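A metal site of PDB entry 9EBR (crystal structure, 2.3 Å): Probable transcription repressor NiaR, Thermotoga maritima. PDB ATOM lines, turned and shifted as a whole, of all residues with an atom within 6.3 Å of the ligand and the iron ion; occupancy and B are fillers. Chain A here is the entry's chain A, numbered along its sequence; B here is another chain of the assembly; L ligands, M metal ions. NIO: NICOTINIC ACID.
OE1 of Glu 87 binds the iron ion (2.2 Å). A ring nitrogen (NE2) of His 79 binds the iron ion (2.2 Å). A ring nitrogen (NE2) of His 148 binds the iron ion (2.3 Å). The iron ion is bound by NE2 of His 146 (2.3 Å). A nitrogen (N) of the ligand is bound to the iron ion, at 2.4 Å. The side-chain carboxylate (OE2) of Glu 87 is bound to the iron ion, at 2.6 Å.
Ile 84 touches the ligand. Val 101 touches the ligand (CG1 to O2, 3.9 Å). CD1 of Ile 115 touches C4 of the ligand (3.7 Å). Phe 126 touches the ligand. Met 130 touches the ligand. Pro 137 touches the ligand. Hydrophobic or aromatic side chains within 4 Å of the ligand: His 79, Ile 84, Val 101, Ile 115, Phe 126, Met 130, Pro 137, Leu 138, Leu 139, His 146, His 148 and Tyr 108 of chain B. The nearest printed residue that does not touch the ligand is Leu 88 (4.1 Å).
N of Leu 139 sits at hydrogen-bond distance from O1 of the ligand, 2.6 Å away. OH of Tyr 108 of chain B is in hydrogen-bond range of O2 of the ligand (2.6 Å). The backbone NH of Leu 138 is in hydrogen-bond range of an oxygen (O2) of the ligand.
OG1 of Thr 140 sits at hydrogen-bond distance from O of Pro 137, 2.5 Å away. A ring nitrogen (ND1) of His 105 of chain B sits at hydrogen-bond distance from the backbone NH of Tyr 108 of chain B, 2.9 Å away. The backbone carbonyl oxygen of Val 77 is in hydrogen-bond range of the backbone NH of His 146 (2.9 Å).
Val 77 touches the iron ion. Of the 22 residues printed, 5 come within 4 Å of the iron ion.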
ATOM      1  N   VAL A  77      -7.657 -31.919 -31.220  1.00  0.00           N
ATOM      2  CA  VAL A  77      -8.111 -32.175 -29.859  1.00  0.00           C
ATOM      3  C   VAL A  77      -9.631 -32.088 -29.817  1.00  0.00           C
ATOM      4  O   VAL A  77     -10.278 -31.678 -30.769  1.00  0.00           O
ATOM      5  CB  VAL A  77      -7.493 -31.191 -28.842  1.00  0.00           C
ATOM      6  CG1 VAL A  77      -5.972 -31.278 -28.884  1.00  0.00           C
ATOM      7  CG2 VAL A  77      -8.008 -29.775 -29.112  1.00  0.00           C
ATOM      8  N   HIS A  79     -12.583 -31.255 -26.476  1.00  0.00           N
ATOM      9  CA  HIS A  79     -12.920 -31.099 -25.067  1.00  0.00           C
ATOM     10  C   HIS A  79     -14.045 -30.088 -24.960  1.00  0.00           C
ATOM     11  O   HIS A  79     -14.363 -29.362 -25.914  1.00  0.00           O
ATOM     12  CB  HIS A  79     -11.712 -30.651 -24.270  1.00  0.00           C
ATOM     13  CG  HIS A  79     -11.150 -29.359 -24.736  1.00  0.00           C
ATOM     14  ND1 HIS A  79     -11.824 -28.167 -24.604  1.00  0.00           N
ATOM     15  CD2 HIS A  79      -9.981 -29.075 -25.357  1.00  0.00           C
ATOM     16  CE1 HIS A  79     -11.099 -27.196 -25.111  1.00  0.00           C
ATOM     17  NE2 HIS A  79      -9.974 -27.719 -25.576  1.00  0.00           N
ATOM     18  N   GLU A  83     -13.172 -27.210 -20.176  1.00  0.00           N
ATOM     19  CA  GLU A  83     -11.838 -27.788 -20.123  1.00  0.00           C
ATOM     20  C   GLU A  83     -10.797 -26.893 -20.796  1.00  0.00           C
ATOM     21  O   GLU A  83      -9.669 -27.364 -21.058  1.00  0.00           O
ATOM     22  CB  GLU A  83     -11.853 -29.172 -20.769  1.00  0.00           C
ATOM     23  CG  GLU A  83     -13.188 -29.913 -20.579  1.00  0.00           C
ATOM     24  CD  GLU A  83     -13.065 -31.428 -20.675  1.00  0.00           C
ATOM     25  OE1 GLU A  83     -12.724 -32.071 -19.676  1.00  0.00           O
ATOM     26  OE2 GLU A  83     -13.340 -31.991 -21.765  1.00  0.00           O
ATOM     27  N   ILE A  84     -11.134 -25.632 -21.098  1.00  0.00           N
ATOM     28  CA  ILE A  84     -10.181 -24.790 -21.805  1.00  0.00           C
ATOM     29  C   ILE A  84      -8.982 -24.473 -20.911  1.00  0.00           C
ATOM     30  O   ILE A  84      -7.829 -24.517 -21.373  1.00  0.00           O
ATOM     31  CB  ILE A  84     -10.859 -23.502 -22.324  1.00  0.00           C
ATOM     32  CG1 ILE A  84     -11.768 -23.833 -23.508  1.00  0.00           C
ATOM     33  CG2 ILE A  84      -9.821 -22.445 -22.730  1.00  0.00           C
ATOM     34  CD1 ILE A  84     -12.632 -22.702 -23.964  1.00  0.00           C
ATOM     35  N   GLU A  87      -6.414 -27.362 -20.564  1.00  0.00           N
ATOM     36  CA  GLU A  87      -5.655 -27.539 -21.794  1.00  0.00           C
ATOM     37  C   GLU A  87      -4.613 -26.442 -21.963  1.00  0.00           C
ATOM     38  O   GLU A  87      -3.433 -26.729 -22.199  1.00  0.00           O
ATOM     39  CB  GLU A  87      -6.603 -27.583 -22.986  1.00  0.00           C
ATOM     40  CG  GLU A  87      -5.884 -27.734 -24.315  1.00  0.00           C
ATOM     41  CD  GLU A  87      -6.769 -27.395 -25.521  1.00  0.00           C
ATOM     42  OE1 GLU A  87      -7.145 -26.236 -25.641  1.00  0.00           O
ATOM     43  OE2 GLU A  87      -7.097 -28.285 -26.347  1.00  0.00           O
ATOM     44  N   LEU A  88      -5.020 -25.182 -21.842  1.00  0.00           N
ATOM     45  CA  LEU A  88      -4.074 -24.088 -22.026  1.00  0.00           C
ATOM     46  C   LEU A  88      -2.949 -24.148 -21.002  1.00  0.00           C
ATOM     47  O   LEU A  88      -1.759 -24.113 -21.366  1.00  0.00           O
ATOM     48  CB  LEU A  88      -4.805 -22.734 -21.978  1.00  0.00           C
ATOM     49  CG  LEU A  88      -5.825 -22.433 -23.095  1.00  0.00           C
ATOM     50  CD1 LEU A  88      -6.379 -20.998 -23.025  1.00  0.00           C
ATOM     51  CD2 LEU A  88      -5.235 -22.691 -24.477  1.00  0.00           C
ATOM     52  N   ILE A  98      -0.011 -21.272 -27.200  1.00  0.00           N
ATOM     53  CA  ILE A  98      -1.211 -21.611 -27.960  1.00  0.00           C
ATOM     54  C   ILE A  98      -1.474 -20.452 -28.908  1.00  0.00           C
ATOM     55  O   ILE A  98      -1.978 -19.422 -28.489  1.00  0.00           O
ATOM     56  CB  ILE A  98      -2.430 -21.888 -27.084  1.00  0.00           C
ATOM     57  CG1 ILE A  98      -2.107 -22.906 -26.005  1.00  0.00           C
ATOM     58  CG2 ILE A  98      -3.611 -22.368 -27.992  1.00  0.00           C
ATOM     59  CD1 ILE A  98      -1.396 -22.301 -24.797  1.00  0.00           C
ATOM     60  N   VAL A 101      -7.031 -21.181 -32.406  1.00  0.00           N
ATOM     61  CA  VAL A 101      -7.947 -22.298 -32.465  1.00  0.00           C
ATOM     62  C   VAL A 101      -8.594 -22.264 -33.831  1.00  0.00           C
ATOM     63  O   VAL A 101      -8.944 -21.192 -34.330  1.00  0.00           O
ATOM     64  CB  VAL A 101      -9.036 -22.239 -31.389  1.00  0.00           C
ATOM     65  CG1 VAL A 101      -9.771 -20.928 -31.466  1.00  0.00           C
ATOM     66  CG2 VAL A 101      -9.997 -23.397 -31.604  1.00  0.00           C
ATOM     67  N   VAL A 103     -11.627 -24.233 -36.028  1.00  0.00           N
ATOM     68  CA  VAL A 103     -12.720 -25.178 -36.142  1.00  0.00           C
ATOM     69  C   VAL A 103     -13.037 -25.408 -37.611  1.00  0.00           C
ATOM     70  O   VAL A 103     -12.988 -24.483 -38.425  1.00  0.00           O
ATOM     71  CB  VAL A 103     -13.936 -24.635 -35.376  1.00  0.00           C
ATOM     72  CG1 VAL A 103     -15.187 -25.362 -35.815  1.00  0.00           C
ATOM     73  CG2 VAL A 103     -13.691 -24.831 -33.899  1.00  0.00           C
ATOM     74  N   ILE A 115      -5.490 -16.729 -30.252  1.00  0.00           N
ATOM     75  CA  ILE A 115      -5.339 -17.030 -28.833  1.00  0.00           C
ATOM     76  C   ILE A 115      -4.048 -16.401 -28.307  1.00  0.00           C
ATOM     77  O   ILE A 115      -4.090 -15.592 -27.375  1.00  0.00           O
ATOM     78  CB  ILE A 115      -5.398 -18.538 -28.584  1.00  0.00           C
ATOM     79  CG1 ILE A 115      -6.766 -19.078 -29.026  1.00  0.00           C
ATOM     80  CG2 ILE A 115      -5.157 -18.886 -27.143  1.00  0.00           C
ATOM     81  CD1 ILE A 115      -6.976 -20.578 -28.718  1.00  0.00           C
ATOM     82  N   PHE A 126      -7.513 -14.989 -20.332  1.00  0.00           N
ATOM     83  CA  PHE A 126      -8.295 -15.554 -21.442  1.00  0.00           C
ATOM     84  C   PHE A 126      -9.500 -16.337 -20.929  1.00  0.00           C
ATOM     85  O   PHE A 126     -10.604 -16.208 -21.472  1.00  0.00           O
ATOM     86  CB  PHE A 126      -7.393 -16.425 -22.310  1.00  0.00           C
ATOM     87  CG  PHE A 126      -8.079 -17.041 -23.506  1.00  0.00           C
ATOM     88  CD1 PHE A 126      -8.803 -18.208 -23.379  1.00  0.00           C
ATOM     89  CD2 PHE A 126      -7.994 -16.438 -24.739  1.00  0.00           C
ATOM     90  CE1 PHE A 126      -9.452 -18.745 -24.477  1.00  0.00           C
ATOM     91  CE2 PHE A 126      -8.635 -17.002 -25.845  1.00  0.00           C
ATOM     92  CZ  PHE A 126      -9.349 -18.154 -25.712  1.00  0.00           C
ATOM     93  N   MET A 130     -13.572 -15.552 -21.587  1.00  0.00           N
ATOM     94  CA  MET A 130     -14.428 -16.569 -22.186  1.00  0.00           C
ATOM     95  C   MET A 130     -15.540 -16.987 -21.234  1.00  0.00           C
ATOM     96  O   MET A 130     -16.673 -17.262 -21.669  1.00  0.00           O
ATOM     97  CB  MET A 130     -13.564 -17.776 -22.581  1.00  0.00           C
ATOM     98  CG  MET A 130     -14.233 -18.748 -23.533  1.00  0.00           C
ATOM     99  SD  MET A 130     -14.492 -18.043 -25.185  1.00  0.00           S
ATOM    100  CE  MET A 130     -12.934 -18.429 -26.036  1.00  0.00           C
ATOM    101  N   GLU A 136     -18.930 -17.532 -26.206  1.00  0.00           N
ATOM    102  CA  GLU A 136     -18.841 -18.973 -26.331  1.00  0.00           C
ATOM    103  C   GLU A 136     -17.636 -19.372 -27.158  1.00  0.00           C
ATOM    104  O   GLU A 136     -17.335 -18.723 -28.170  1.00  0.00           O
ATOM    105  CB  GLU A 136     -20.103 -19.521 -26.999  1.00  0.00           C
ATOM    106  CG  GLU A 136     -21.337 -19.005 -26.331  1.00  0.00           C
ATOM    107  CD  GLU A 136     -21.500 -19.602 -24.959  1.00  0.00           C
ATOM    108  OE1 GLU A 136     -21.116 -20.772 -24.789  1.00  0.00           O
ATOM    109  OE2 GLU A 136     -21.995 -18.881 -24.054  1.00  0.00           O
ATOM    110  N   PRO A 137     -16.926 -20.437 -26.791  1.00  0.00           N
ATOM    111  CA  PRO A 137     -15.722 -20.824 -27.540  1.00  0.00           C
ATOM    112  C   PRO A 137     -16.090 -21.403 -28.901  1.00  0.00           C
ATOM    113  O   PRO A 137     -17.192 -21.906 -29.119  1.00  0.00           O
ATOM    114  CB  PRO A 137     -15.061 -21.876 -26.650  1.00  0.00           C
ATOM    115  CG  PRO A 137     -15.819 -21.822 -25.329  1.00  0.00           C
ATOM    116  CD  PRO A 137     -17.174 -21.316 -25.640  1.00  0.00           C
ATOM    117  N   LEU A 138     -15.129 -21.346 -29.828  1.00  0.00           N
ATOM    118  CA  LEU A 138     -15.402 -21.844 -31.175  1.00  0.00           C
ATOM    119  C   LEU A 138     -15.801 -23.319 -31.163  1.00  0.00           C
ATOM    120  O   LEU A 138     -16.664 -23.726 -31.945  1.00  0.00           O
ATOM    121  CB  LEU A 138     -14.193 -21.598 -32.089  1.00  0.00           C
ATOM    122  CG  LEU A 138     -13.878 -20.120 -32.299  1.00  0.00           C
ATOM    123  CD1 LEU A 138     -12.804 -19.844 -33.348  1.00  0.00           C
ATOM    124  CD2 LEU A 138     -15.162 -19.388 -32.663  1.00  0.00           C
ATOM    125  N   LEU A 139     -15.231 -24.130 -30.262  1.00  0.00           N
ATOM    126  CA  LEU A 139     -15.545 -25.562 -30.254  1.00  0.00           C
ATOM    127  C   LEU A 139     -17.050 -25.824 -30.126  1.00  0.00           C
ATOM    128  O   LEU A 139     -17.480 -26.960 -30.388  1.00  0.00           O
ATOM    129  CB  LEU A 139     -14.785 -26.272 -29.123  1.00  0.00           C
ATOM    130  CG  LEU A 139     -15.006 -25.797 -27.689  1.00  0.00           C
ATOM    131  CD1 LEU A 139     -16.174 -26.514 -27.045  1.00  0.00           C
ATOM    132  CD2 LEU A 139     -13.743 -25.923 -26.830  1.00  0.00           C
ATOM    133  N   THR A 140     -17.848 -24.818 -29.765  1.00  0.00           N
ATOM    134  CA  THR A 140     -19.290 -25.040 -29.662  1.00  0.00           C
ATOM    135  C   THR A 140     -19.950 -25.114 -31.023  1.00  0.00           C
ATOM    136  O   THR A 140     -21.063 -25.648 -31.135  1.00  0.00           O
ATOM    137  CB  THR A 140     -19.931 -23.944 -28.797  1.00  0.00           C
ATOM    138  OG1 THR A 140     -19.548 -22.657 -29.286  1.00  0.00           O
ATOM    139  CG2 THR A 140     -19.481 -24.080 -27.362  1.00  0.00           C
ATOM    140  N   HIS A 146     -11.718 -29.737 -32.431  1.00  0.00           N
ATOM    141  CA  HIS A 146     -11.139 -28.550 -33.034  1.00  0.00           C
ATOM    142  C   HIS A 146      -9.635 -28.725 -33.084  1.00  0.00           C
ATOM    143  O   HIS A 146      -9.090 -29.684 -32.542  1.00  0.00           O
ATOM    144  CB  HIS A 146     -11.493 -27.302 -32.237  1.00  0.00           C
ATOM    145  CG  HIS A 146     -10.994 -27.320 -30.834  1.00  0.00           C
ATOM    146  ND1 HIS A 146     -11.562 -28.125 -29.855  1.00  0.00           N
ATOM    147  CD2 HIS A 146      -9.993 -26.644 -30.218  1.00  0.00           C
ATOM    148  CE1 HIS A 146     -10.936 -27.923 -28.712  1.00  0.00           C
ATOM    149  NE2 HIS A 146      -9.986 -27.021 -28.905  1.00  0.00           N
ATOM    150  N   LEU A 147      -8.964 -27.727 -33.664  1.00  0.00           N
ATOM    151  CA  LEU A 147      -7.527 -27.750 -33.826  1.00  0.00           C
ATOM    152  C   LEU A 147      -6.906 -26.606 -33.043  1.00  0.00           C
ATOM    153  O   LEU A 147      -7.542 -25.575 -32.790  1.00  0.00           O
ATOM    154  CB  LEU A 147      -7.131 -27.641 -35.305  1.00  0.00           C
ATOM    155  CG  LEU A 147      -7.708 -28.696 -36.245  1.00  0.00           C
ATOM    156  CD1 LEU A 147      -7.468 -28.316 -37.702  1.00  0.00           C
ATOM    157  CD2 LEU A 147      -7.153 -30.087 -35.979  1.00  0.00           C
ATOM    158  N   HIS A 148      -5.648 -26.784 -32.668  1.00  0.00           N
ATOM    159  CA  HIS A 148      -4.840 -25.691 -32.149  1.00  0.00           C
ATOM    160  C   HIS A 148      -3.521 -25.662 -32.896  1.00  0.00           C
ATOM    161  O   HIS A 148      -2.990 -26.716 -33.268  1.00  0.00           O
ATOM    162  CB  HIS A 148      -4.590 -25.858 -30.658  1.00  0.00           C
ATOM    163  CG  HIS A 148      -5.749 -25.475 -29.808  1.00  0.00           C
ATOM    164  ND1 HIS A 148      -6.292 -24.213 -29.811  1.00  0.00           N
ATOM    165  CD2 HIS A 148      -6.459 -26.191 -28.901  1.00  0.00           C
ATOM    166  CE1 HIS A 148      -7.292 -24.163 -28.959  1.00  0.00           C
ATOM    167  NE2 HIS A 148      -7.394 -25.339 -28.373  1.00  0.00           N
ATOM    168  N   HIS B 105     -16.931 -11.190 -31.933  1.00  0.00           N
ATOM    169  CA  HIS B 105     -16.740 -12.062 -30.786  1.00  0.00           C
ATOM    170  C   HIS B 105     -15.952 -11.341 -29.695  1.00  0.00           C
ATOM    171  O   HIS B 105     -14.864 -10.814 -29.976  1.00  0.00           O
ATOM    172  CB  HIS B 105     -16.027 -13.342 -31.212  1.00  0.00           C
ATOM    173  CG  HIS B 105     -15.943 -14.392 -30.141  1.00  0.00           C
ATOM    174  ND1 HIS B 105     -15.111 -14.257 -29.040  1.00  0.00           N
ATOM    175  CD2 HIS B 105     -16.581 -15.578 -29.993  1.00  0.00           C
ATOM    176  CE1 HIS B 105     -15.237 -15.328 -28.276  1.00  0.00           C
ATOM    177  NE2 HIS B 105     -16.128 -16.132 -28.826  1.00  0.00           N
ATOM    178  N   TYR B 108     -12.418 -13.197 -29.510  1.00  0.00           N
ATOM    179  CA  TYR B 108     -11.703 -13.331 -30.774  1.00  0.00           C
ATOM    180  C   TYR B 108     -11.868 -12.141 -31.717  1.00  0.00           C
ATOM    181  O   TYR B 108     -11.169 -12.057 -32.732  1.00  0.00           O
ATOM    182  CB  TYR B 108     -12.170 -14.591 -31.469  1.00  0.00           C
ATOM    183  CG  TYR B 108     -11.829 -15.829 -30.705  1.00  0.00           C
ATOM    184  CD1 TYR B 108     -10.534 -16.003 -30.167  1.00  0.00           C
ATOM    185  CD2 TYR B 108     -12.759 -16.822 -30.513  1.00  0.00           C
ATOM    186  CE1 TYR B 108     -10.219 -17.156 -29.483  1.00  0.00           C
ATOM    187  CE2 TYR B 108     -12.436 -17.973 -29.815  1.00  0.00           C
ATOM    188  CZ  TYR B 108     -11.184 -18.117 -29.309  1.00  0.00           C
ATOM    189  OH  TYR B 108     -10.896 -19.257 -28.606  1.00  0.00           O
HETATM  190  N   NIO L   1      -9.589 -24.215 -26.846  1.00  0.00           N
HETATM  191  C1  NIO L   1     -10.702 -23.975 -27.573  1.00  0.00           C
HETATM  192  C2  NIO L   1     -11.191 -22.683 -27.660  1.00  0.00           C
HETATM  193  C3  NIO L   1     -10.524 -21.690 -27.011  1.00  0.00           C
HETATM  194  C4  NIO L   1      -9.391 -21.956 -26.285  1.00  0.00           C
HETATM  195  C5  NIO L   1      -8.909 -23.256 -26.200  1.00  0.00           C
HETATM  196  C6  NIO L   1     -12.444 -22.348 -28.480  1.00  0.00           C
HETATM  197  O1  NIO L   1     -13.270 -23.229 -28.840  1.00  0.00           O
HETATM  198  O2  NIO L   1     -12.642 -21.154 -28.836  1.00  0.00           O
HETATM  199 FE    FE M   1      -8.806 -26.472 -27.014  1.00  0.00          FE
